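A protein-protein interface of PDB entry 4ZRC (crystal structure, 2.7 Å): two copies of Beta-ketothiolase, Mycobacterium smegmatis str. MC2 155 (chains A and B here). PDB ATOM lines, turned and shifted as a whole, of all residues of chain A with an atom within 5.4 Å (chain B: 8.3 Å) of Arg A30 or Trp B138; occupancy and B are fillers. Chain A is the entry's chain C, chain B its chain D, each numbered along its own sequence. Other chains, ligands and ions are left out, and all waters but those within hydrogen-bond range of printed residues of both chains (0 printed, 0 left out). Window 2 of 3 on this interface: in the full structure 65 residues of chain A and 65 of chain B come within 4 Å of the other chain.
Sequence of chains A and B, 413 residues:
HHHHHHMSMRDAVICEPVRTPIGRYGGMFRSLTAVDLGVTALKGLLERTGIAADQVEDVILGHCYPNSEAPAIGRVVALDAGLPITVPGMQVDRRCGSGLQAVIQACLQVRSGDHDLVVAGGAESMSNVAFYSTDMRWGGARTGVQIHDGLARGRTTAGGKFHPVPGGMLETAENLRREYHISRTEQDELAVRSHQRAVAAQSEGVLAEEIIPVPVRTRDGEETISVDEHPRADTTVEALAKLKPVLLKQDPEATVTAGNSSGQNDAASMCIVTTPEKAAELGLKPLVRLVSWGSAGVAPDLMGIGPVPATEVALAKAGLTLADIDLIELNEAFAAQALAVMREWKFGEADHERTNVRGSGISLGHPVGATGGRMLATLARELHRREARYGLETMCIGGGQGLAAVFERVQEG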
ATOM      1  N   TYR A  25      25.733  18.999  -0.350  1.00  0.00           N
ATOM      2  CA  TYR A  25      25.005  18.156  -1.275  1.00  0.00           C
ATOM      3  C   TYR A  25      25.675  18.242  -2.672  1.00  0.00           C
ATOM      4  O   TYR A  25      25.670  19.293  -3.320  1.00  0.00           O
ATOM      5  CB  TYR A  25      23.513  18.553  -1.291  1.00  0.00           C
ATOM      6  CG  TYR A  25      22.660  18.012  -2.419  1.00  0.00           C
ATOM      7  CD1 TYR A  25      23.198  17.655  -3.627  1.00  0.00           C
ATOM      8  CD2 TYR A  25      21.307  17.914  -2.301  1.00  0.00           C
ATOM      9  CE1 TYR A  25      22.419  17.182  -4.662  1.00  0.00           C
ATOM     10  CE2 TYR A  25      20.525  17.443  -3.352  1.00  0.00           C
ATOM     11  CZ  TYR A  25      21.102  17.071  -4.526  1.00  0.00           C
ATOM     12  OH  TYR A  25      20.394  16.599  -5.594  1.00  0.00           O
ATOM     13  N   GLY A  26      26.253  17.130  -3.123  1.00  0.00           N
ATOM     14  CA  GLY A  26      26.893  17.084  -4.420  1.00  0.00           C
ATOM     15  C   GLY A  26      28.339  17.523  -4.319  1.00  0.00           C
ATOM     16  O   GLY A  26      28.952  17.885  -5.327  1.00  0.00           O
ATOM     17  N   GLY A  27      28.873  17.488  -3.096  1.00  0.00           N
ATOM     18  CA  GLY A  27      30.233  17.930  -2.822  1.00  0.00           C
ATOM     19  C   GLY A  27      31.211  16.805  -2.563  1.00  0.00           C
ATOM     20  O   GLY A  27      31.123  15.765  -3.182  1.00  0.00           O
ATOM     21  N   MET A  28      32.119  17.024  -1.614  1.00  0.00           N
ATOM     22  CA  MET A  28      33.250  16.135  -1.344  1.00  0.00           C
ATOM     23  C   MET A  28      32.900  14.735  -0.889  1.00  0.00           C
ATOM     24  O   MET A  28      33.688  13.817  -1.123  1.00  0.00           O
ATOM     25  CB  MET A  28      34.204  16.755  -0.324  1.00  0.00           C
ATOM     26  CG  MET A  28      33.627  16.914   1.071  1.00  0.00           C
ATOM     27  SD  MET A  28      34.549  18.090   2.066  1.00  0.00           S
ATOM     28  CE  MET A  28      33.831  17.877   3.688  1.00  0.00           C
ATOM     29  N   PHE A  29      31.750  14.561  -0.228  1.00  0.00           N
ATOM     30  CA  PHE A  29      31.355  13.228   0.244  1.00  0.00           C
ATOM     31  C   PHE A  29      30.312  12.526  -0.628  1.00  0.00           C
ATOM     32  O   PHE A  29      29.769  11.490  -0.219  1.00  0.00           O
ATOM     33  CB  PHE A  29      30.916  13.240   1.716  1.00  0.00           C
ATOM     34  CG  PHE A  29      32.018  13.557   2.677  1.00  0.00           C
ATOM     35  CD1 PHE A  29      33.266  12.974   2.530  1.00  0.00           C
ATOM     36  CD2 PHE A  29      31.808  14.431   3.724  1.00  0.00           C
ATOM     37  CE1 PHE A  29      34.291  13.261   3.403  1.00  0.00           C
ATOM     38  CE2 PHE A  29      32.827  14.728   4.604  1.00  0.00           C
ATOM     39  CZ  PHE A  29      34.068  14.138   4.449  1.00  0.00           C
ATOM     40  N   ARG A  30      30.075  13.065  -1.834  1.00  0.00           N
ATOM     41  CA  ARG A  30      29.143  12.506  -2.828  1.00  0.00           C
ATOM     42  C   ARG A  30      29.339  11.015  -3.192  1.00  0.00           C
ATOM     43  O   ARG A  30      28.370  10.313  -3.421  1.00  0.00           O
ATOM     44  CB  ARG A  30      29.148  13.374  -4.077  1.00  0.00           C
ATOM     45  CG  ARG A  30      28.322  12.845  -5.239  1.00  0.00           C
ATOM     46  CD  ARG A  30      28.170  13.950  -6.249  1.00  0.00           C
ATOM     47  NE  ARG A  30      28.291  13.476  -7.612  1.00  0.00           N
ATOM     48  CZ  ARG A  30      28.281  14.286  -8.663  1.00  0.00           C
ATOM     49  NH1 ARG A  30      28.173  15.604  -8.478  1.00  0.00           N
ATOM     50  NH2 ARG A  30      28.387  13.785  -9.893  1.00  0.00           N
ATOM     51  N   SER A  31      30.584  10.549  -3.249  1.00  0.00           N
ATOM     52  CA  SER A  31      30.895   9.129  -3.456  1.00  0.00           C
ATOM     53  C   SER A  31      30.562   8.254  -2.248  1.00  0.00           C
ATOM     54  O   SER A  31      30.589   7.060  -2.355  1.00  0.00           O
ATOM     55  CB  SER A  31      32.388   8.956  -3.756  1.00  0.00           C
ATOM     56  OG  SER A  31      33.187   9.673  -2.844  1.00  0.00           O
ATOM     57  N   LEU A  32      30.275   8.843  -1.090  1.00  0.00           N
ATOM     58  CA  LEU A  32      30.108   8.045   0.131  1.00  0.00           C
ATOM     59  C   LEU A  32      28.659   7.912   0.597  1.00  0.00           C
ATOM     60  O   LEU A  32      27.910   8.883   0.564  1.00  0.00           O
ATOM     61  CB  LEU A  32      30.953   8.611   1.280  1.00  0.00           C
ATOM     62  CG  LEU A  32      32.476   8.637   1.180  1.00  0.00           C
ATOM     63  CD1 LEU A  32      32.939   9.629   2.222  1.00  0.00           C
ATOM     64  CD2 LEU A  32      33.121   7.271   1.419  1.00  0.00           C
ATOM     65  N   SER A 127      23.223  13.607  -0.500  1.00  0.00           N
ATOM     66  CA  SER A 127      23.672  13.416  -1.858  1.00  0.00           C
ATOM     67  C   SER A 127      23.141  12.146  -2.489  1.00  0.00           C
ATOM     68  O   SER A 127      23.053  12.057  -3.716  1.00  0.00           O
ATOM     69  CB  SER A 127      25.191  13.351  -1.884  1.00  0.00           C
ATOM     70  OG  SER A 127      25.762  14.630  -1.738  1.00  0.00           O
ATOM     71  N   ASN A 128      22.804  11.172  -1.646  1.00  0.00           N
ATOM     72  CA  ASN A 128      22.508   9.826  -2.095  1.00  0.00           C
ATOM     73  C   ASN A 128      21.106   9.315  -1.754  1.00  0.00           C
ATOM     74  O   ASN A 128      20.825   8.122  -1.887  1.00  0.00           O
ATOM     75  CB  ASN A 128      23.623   8.887  -1.632  1.00  0.00           C
ATOM     76  CG  ASN A 128      24.868   9.045  -2.467  1.00  0.00           C
ATOM     77  OD1 ASN A 128      24.809   9.368  -3.555  1.00  0.00           O
ATOM     78  ND2 ASN A 128      25.946   8.805  -1.957  1.00  0.00           N
ATOM     79  N   ASP A 266      25.960  16.384   3.727  1.00  0.00           N
ATOM     80  CA  ASP A 266      26.423  15.042   4.076  1.00  0.00           C
ATOM     81  C   ASP A 266      27.252  15.046   5.372  1.00  0.00           C
ATOM     82  O   ASP A 266      28.144  15.874   5.522  1.00  0.00           O
ATOM     83  CB  ASP A 266      27.266  14.483   2.932  1.00  0.00           C
ATOM     84  CG  ASP A 266      26.450  14.172   1.682  1.00  0.00           C
ATOM     85  OD1 ASP A 266      25.211  14.201   1.736  1.00  0.00           O
ATOM     86  OD2 ASP A 266      27.049  13.859   0.635  1.00  0.00           O
ATOM     87  N   THR B 134      19.102   4.643  -6.338  1.00  0.00           N
ATOM     88  CA  THR B 134      20.163   5.535  -5.928  1.00  0.00           C
ATOM     89  C   THR B 134      21.065   5.978  -7.088  1.00  0.00           C
ATOM     90  O   THR B 134      22.106   6.557  -6.837  1.00  0.00           O
ATOM     91  CB  THR B 134      21.001   4.944  -4.766  1.00  0.00           C
ATOM     92  OG1 THR B 134      21.584   3.701  -5.159  1.00  0.00           O
ATOM     93  CG2 THR B 134      20.153   4.713  -3.565  1.00  0.00           C
ATOM     94  N   ASP B 135      20.594   5.771  -8.326  1.00  0.00           N
ATOM     95  CA  ASP B 135      21.294   6.038  -9.609  1.00  0.00           C
ATOM     96  C   ASP B 135      20.716   7.210 -10.414  1.00  0.00           C
ATOM     97  O   ASP B 135      21.358   7.706 -11.359  1.00  0.00           O
ATOM     98  CB  ASP B 135      21.208   4.814 -10.541  1.00  0.00           C
ATOM     99  CG  ASP B 135      21.800   3.554  -9.936  1.00  0.00           C
ATOM    100  OD1 ASP B 135      22.947   3.654  -9.436  1.00  0.00           O
ATOM    101  OD2 ASP B 135      21.137   2.482  -9.984  1.00  0.00           O
ATOM    102  N   MET B 136      19.492   7.615 -10.070  1.00  0.00           N
ATOM    103  CA  MET B 136      18.765   8.625 -10.819  1.00  0.00           C
ATOM    104  C   MET B 136      19.160  10.090 -10.550  1.00  0.00           C
ATOM    105  O   MET B 136      18.782  10.957 -11.322  1.00  0.00           O
ATOM    106  CB  MET B 136      17.274   8.448 -10.626  1.00  0.00           C
ATOM    107  CG  MET B 136      16.836   7.106 -11.050  1.00  0.00           C
ATOM    108  SD  MET B 136      15.075   6.962 -10.913  1.00  0.00           S
ATOM    109  CE  MET B 136      14.948   5.320 -11.600  1.00  0.00           C
ATOM    110  N   ARG B 137      19.931  10.339  -9.494  1.00  0.00           N
ATOM    111  CA  ARG B 137      20.305  11.702  -9.073  1.00  0.00           C
ATOM    112  C   ARG B 137      21.498  12.306  -9.841  1.00  0.00           C
ATOM    113  O   ARG B 137      21.431  13.438 -10.351  1.00  0.00           O
ATOM    114  CB  ARG B 137      20.552  11.726  -7.568  1.00  0.00           C
ATOM    115  CG  ARG B 137      20.640  13.114  -6.999  1.00  0.00           C
ATOM    116  CD  ARG B 137      20.829  13.089  -5.483  1.00  0.00           C
ATOM    117  NE  ARG B 137      19.694  12.528  -4.768  1.00  0.00           N
ATOM    118  CZ  ARG B 137      18.536  13.146  -4.530  1.00  0.00           C
ATOM    119  NH1 ARG B 137      18.281  14.390  -4.964  1.00  0.00           N
ATOM    120  NH2 ARG B 137      17.601  12.476  -3.869  1.00  0.00           N
ATOM    121  N   TRP B 138      22.583  11.547  -9.936  1.00  0.00           N
ATOM    122  CA  TRP B 138      23.764  12.006 -10.671  1.00  0.00           C
ATOM    123  C   TRP B 138      23.851  11.410 -12.066  1.00  0.00           C
ATOM    124  O   TRP B 138      24.761  11.731 -12.831  1.00  0.00           O
ATOM    125  CB  TRP B 138      25.039  11.819  -9.829  1.00  0.00           C
ATOM    126  CG  TRP B 138      24.798  12.335  -8.420  1.00  0.00           C
ATOM    127  CD1 TRP B 138      24.678  11.589  -7.279  1.00  0.00           C
ATOM    128  CD2 TRP B 138      24.564  13.709  -8.026  1.00  0.00           C
ATOM    129  NE1 TRP B 138      24.411  12.399  -6.211  1.00  0.00           N
ATOM    130  CE2 TRP B 138      24.326  13.704  -6.634  1.00  0.00           C
ATOM    131  CE3 TRP B 138      24.556  14.941  -8.713  1.00  0.00           C
ATOM    132  CZ2 TRP B 138      24.107  14.894  -5.901  1.00  0.00           C
ATOM    133  CZ3 TRP B 138      24.308  16.120  -7.993  1.00  0.00           C
ATOM    134  CH2 TRP B 138      24.105  16.081  -6.603  1.00  0.00           C
ATOM    135  N   GLY B 139      22.866  10.553 -12.373  1.00  0.00           N
ATOM    136  CA  GLY B 139      22.698   9.907 -13.676  1.00  0.00           C
ATOM    137  C   GLY B 139      23.436   8.597 -13.951  1.00  0.00           C
ATOM    138  O   GLY B 139      24.541   8.346 -13.437  1.00  0.00           O
ATOM    139  N   GLY B 140      22.827   7.793 -14.814  1.00  0.00           N
ATOM    140  CA  GLY B 140      23.245   6.426 -15.016  1.00  0.00           C
ATOM    141  C   GLY B 140      24.042   6.150 -16.257  1.00  0.00           C
ATOM    142  O   GLY B 140      23.991   5.041 -16.762  1.00  0.00           O
ATOM    143  N   ALA B 141      24.780   7.148 -16.747  1.00  0.00           N
ATOM    144  CA  ALA B 141      25.654   6.965 -17.925  1.00  0.00           C
ATOM    145  C   ALA B 141      26.697   5.846 -17.696  1.00  0.00           C
ATOM    146  O   ALA B 141      26.685   4.791 -18.356  1.00  0.00           O
ATOM    147  CB  ALA B 141      26.330   8.284 -18.317  1.00  0.00           C
ATOM    148  N   ARG B 142      27.573   6.084 -16.728  1.00  0.00           N
ATOM    149  CA  ARG B 142      28.636   5.143 -16.397  1.00  0.00           C
ATOM    150  C   ARG B 142      28.023   3.773 -16.025  1.00  0.00           C
ATOM    151  O   ARG B 142      28.491   2.736 -16.464  1.00  0.00           O
ATOM    152  CB  ARG B 142      29.504   5.643 -15.193  1.00  0.00           C
ATOM    153  CG  ARG B 142      30.707   6.592 -15.361  1.00  0.00           C
ATOM    154  CD  ARG B 142      31.171   6.830 -16.792  1.00  0.00           C
ATOM    155  NE  ARG B 142      32.553   7.321 -16.895  1.00  0.00           N
ATOM    156  CZ  ARG B 142      33.622   6.549 -17.120  1.00  0.00           C
ATOM    157  NH1 ARG B 142      33.490   5.235 -17.254  1.00  0.00           N
ATOM    158  NH2 ARG B 142      34.832   7.098 -17.217  1.00  0.00           N
ATOM    159  N   THR B 143      26.950   3.804 -15.239  1.00  0.00           N
ATOM    160  CA  THR B 143      26.613   2.718 -14.319  1.00  0.00           C
ATOM    161  C   THR B 143      25.345   1.932 -14.659  1.00  0.00           C
ATOM    162  O   THR B 143      25.133   0.829 -14.152  1.00  0.00           O
ATOM    163  CB  THR B 143      26.450   3.295 -12.895  1.00  0.00           C
ATOM    164  OG1 THR B 143      25.511   4.385 -12.927  1.00  0.00           O
ATOM    165  CG2 THR B 143      27.780   3.812 -12.372  1.00  0.00           C
ATOM    166  N   VAL B 145      21.003   2.186 -14.582  1.00  0.00           N
ATOM    167  CA  VAL B 145      20.116   2.524 -13.482  1.00  0.00           C
ATOM    168  C   VAL B 145      19.462   1.279 -12.922  1.00  0.00           C
ATOM    169  O   VAL B 145      18.817   0.551 -13.670  1.00  0.00           O
ATOM    170  CB  VAL B 145      19.056   3.555 -13.931  1.00  0.00           C
ATOM    171  CG1 VAL B 145      18.070   3.921 -12.807  1.00  0.00           C
ATOM    172  CG2 VAL B 145      19.763   4.787 -14.462  1.00  0.00           C
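NH1 of Arg B137 sits at hydrogen-bond distance from OH of Tyr A25. The indole nitrogen (NE1) of Trp B138 sits at hydrogen-bond distance from the backbone carbonyl oxygen (O) of Ser A127.
Of the 11 printed residues of chain B, 3 touch a printed residue of chain A. Printed residues of chain B that touch a printed residue of chain A: Thr B134, Arg B137 and Trp B138. Hydrophobic or aromatic side chains of chain B within 4 Å of the printed part of chain A: Trp B138. Printed residues of chain A that touch a printed residue of chain B: Tyr A25, Gly A26, Arg A30, Ser A127 and Asn A128. Among the printed residues, no Asp or Glu carboxylate lies within 4 Å of a Lys or Arg side-chain nitrogen of the other chain.
Of chain B, only Trp B138 (3.7 Å) comes within 4 Å of Arg A30. Of chain A, only Tyr A25 (2.8 Å), Gly A26 (3.7 Å), Arg A30 (3.7 Å) and Ser A127 (2.9 Å) come within 4 Å of Trp B138. No residue of chain B comes within 4 Å of Ser A31. Printed residues of chain A within 4 Å of Thr B134: Asn A128 (3.9 Å). Of the printed residues of chain B, Ser A127 touches Arg B137 (3.0 Å) and Trp B138 (2.9 Å). Of the printed residues of chain B, Asn A128 touches Thr B134 (3.9 Å). Ala B141 touches none of the printed residues of chain A. The nearest residue of chain A that does not touch Trp B138 is Asn A128 (4.05 Å). The nearest printed residue of chain B that does not touch Ser A127 is Thr B134 (6.4 Å).
No position is printed for both chains. Of the 7 pairs that touch across the chains among the printed residues, none has its exchanged pair printed and touching as well.
N of Gly A26 is in hydrogen-bond range of OG of Ser A127, at 2.9 Å. OD2 of Asp A266 lies within hydrogen-bond range of OG of Ser A127. The backbone carbonyl oxygen (O) of Arg A30 is in hydrogen-bond range of the side-chain amide nitrogen (ND2) of Asn A128 (3.2 Å). O of Leu A32 is in hydrogen-bond range of ND2 of Asn A128 (3.2 Å).
Among the printed residues, pairs that only touch across the chains: Tyr A25 with Trp B138, Ser A127 with Arg B137, Gly A26 with Trp B138, Arg A30 with Trp B138 and Asn A128 with Thr B134.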
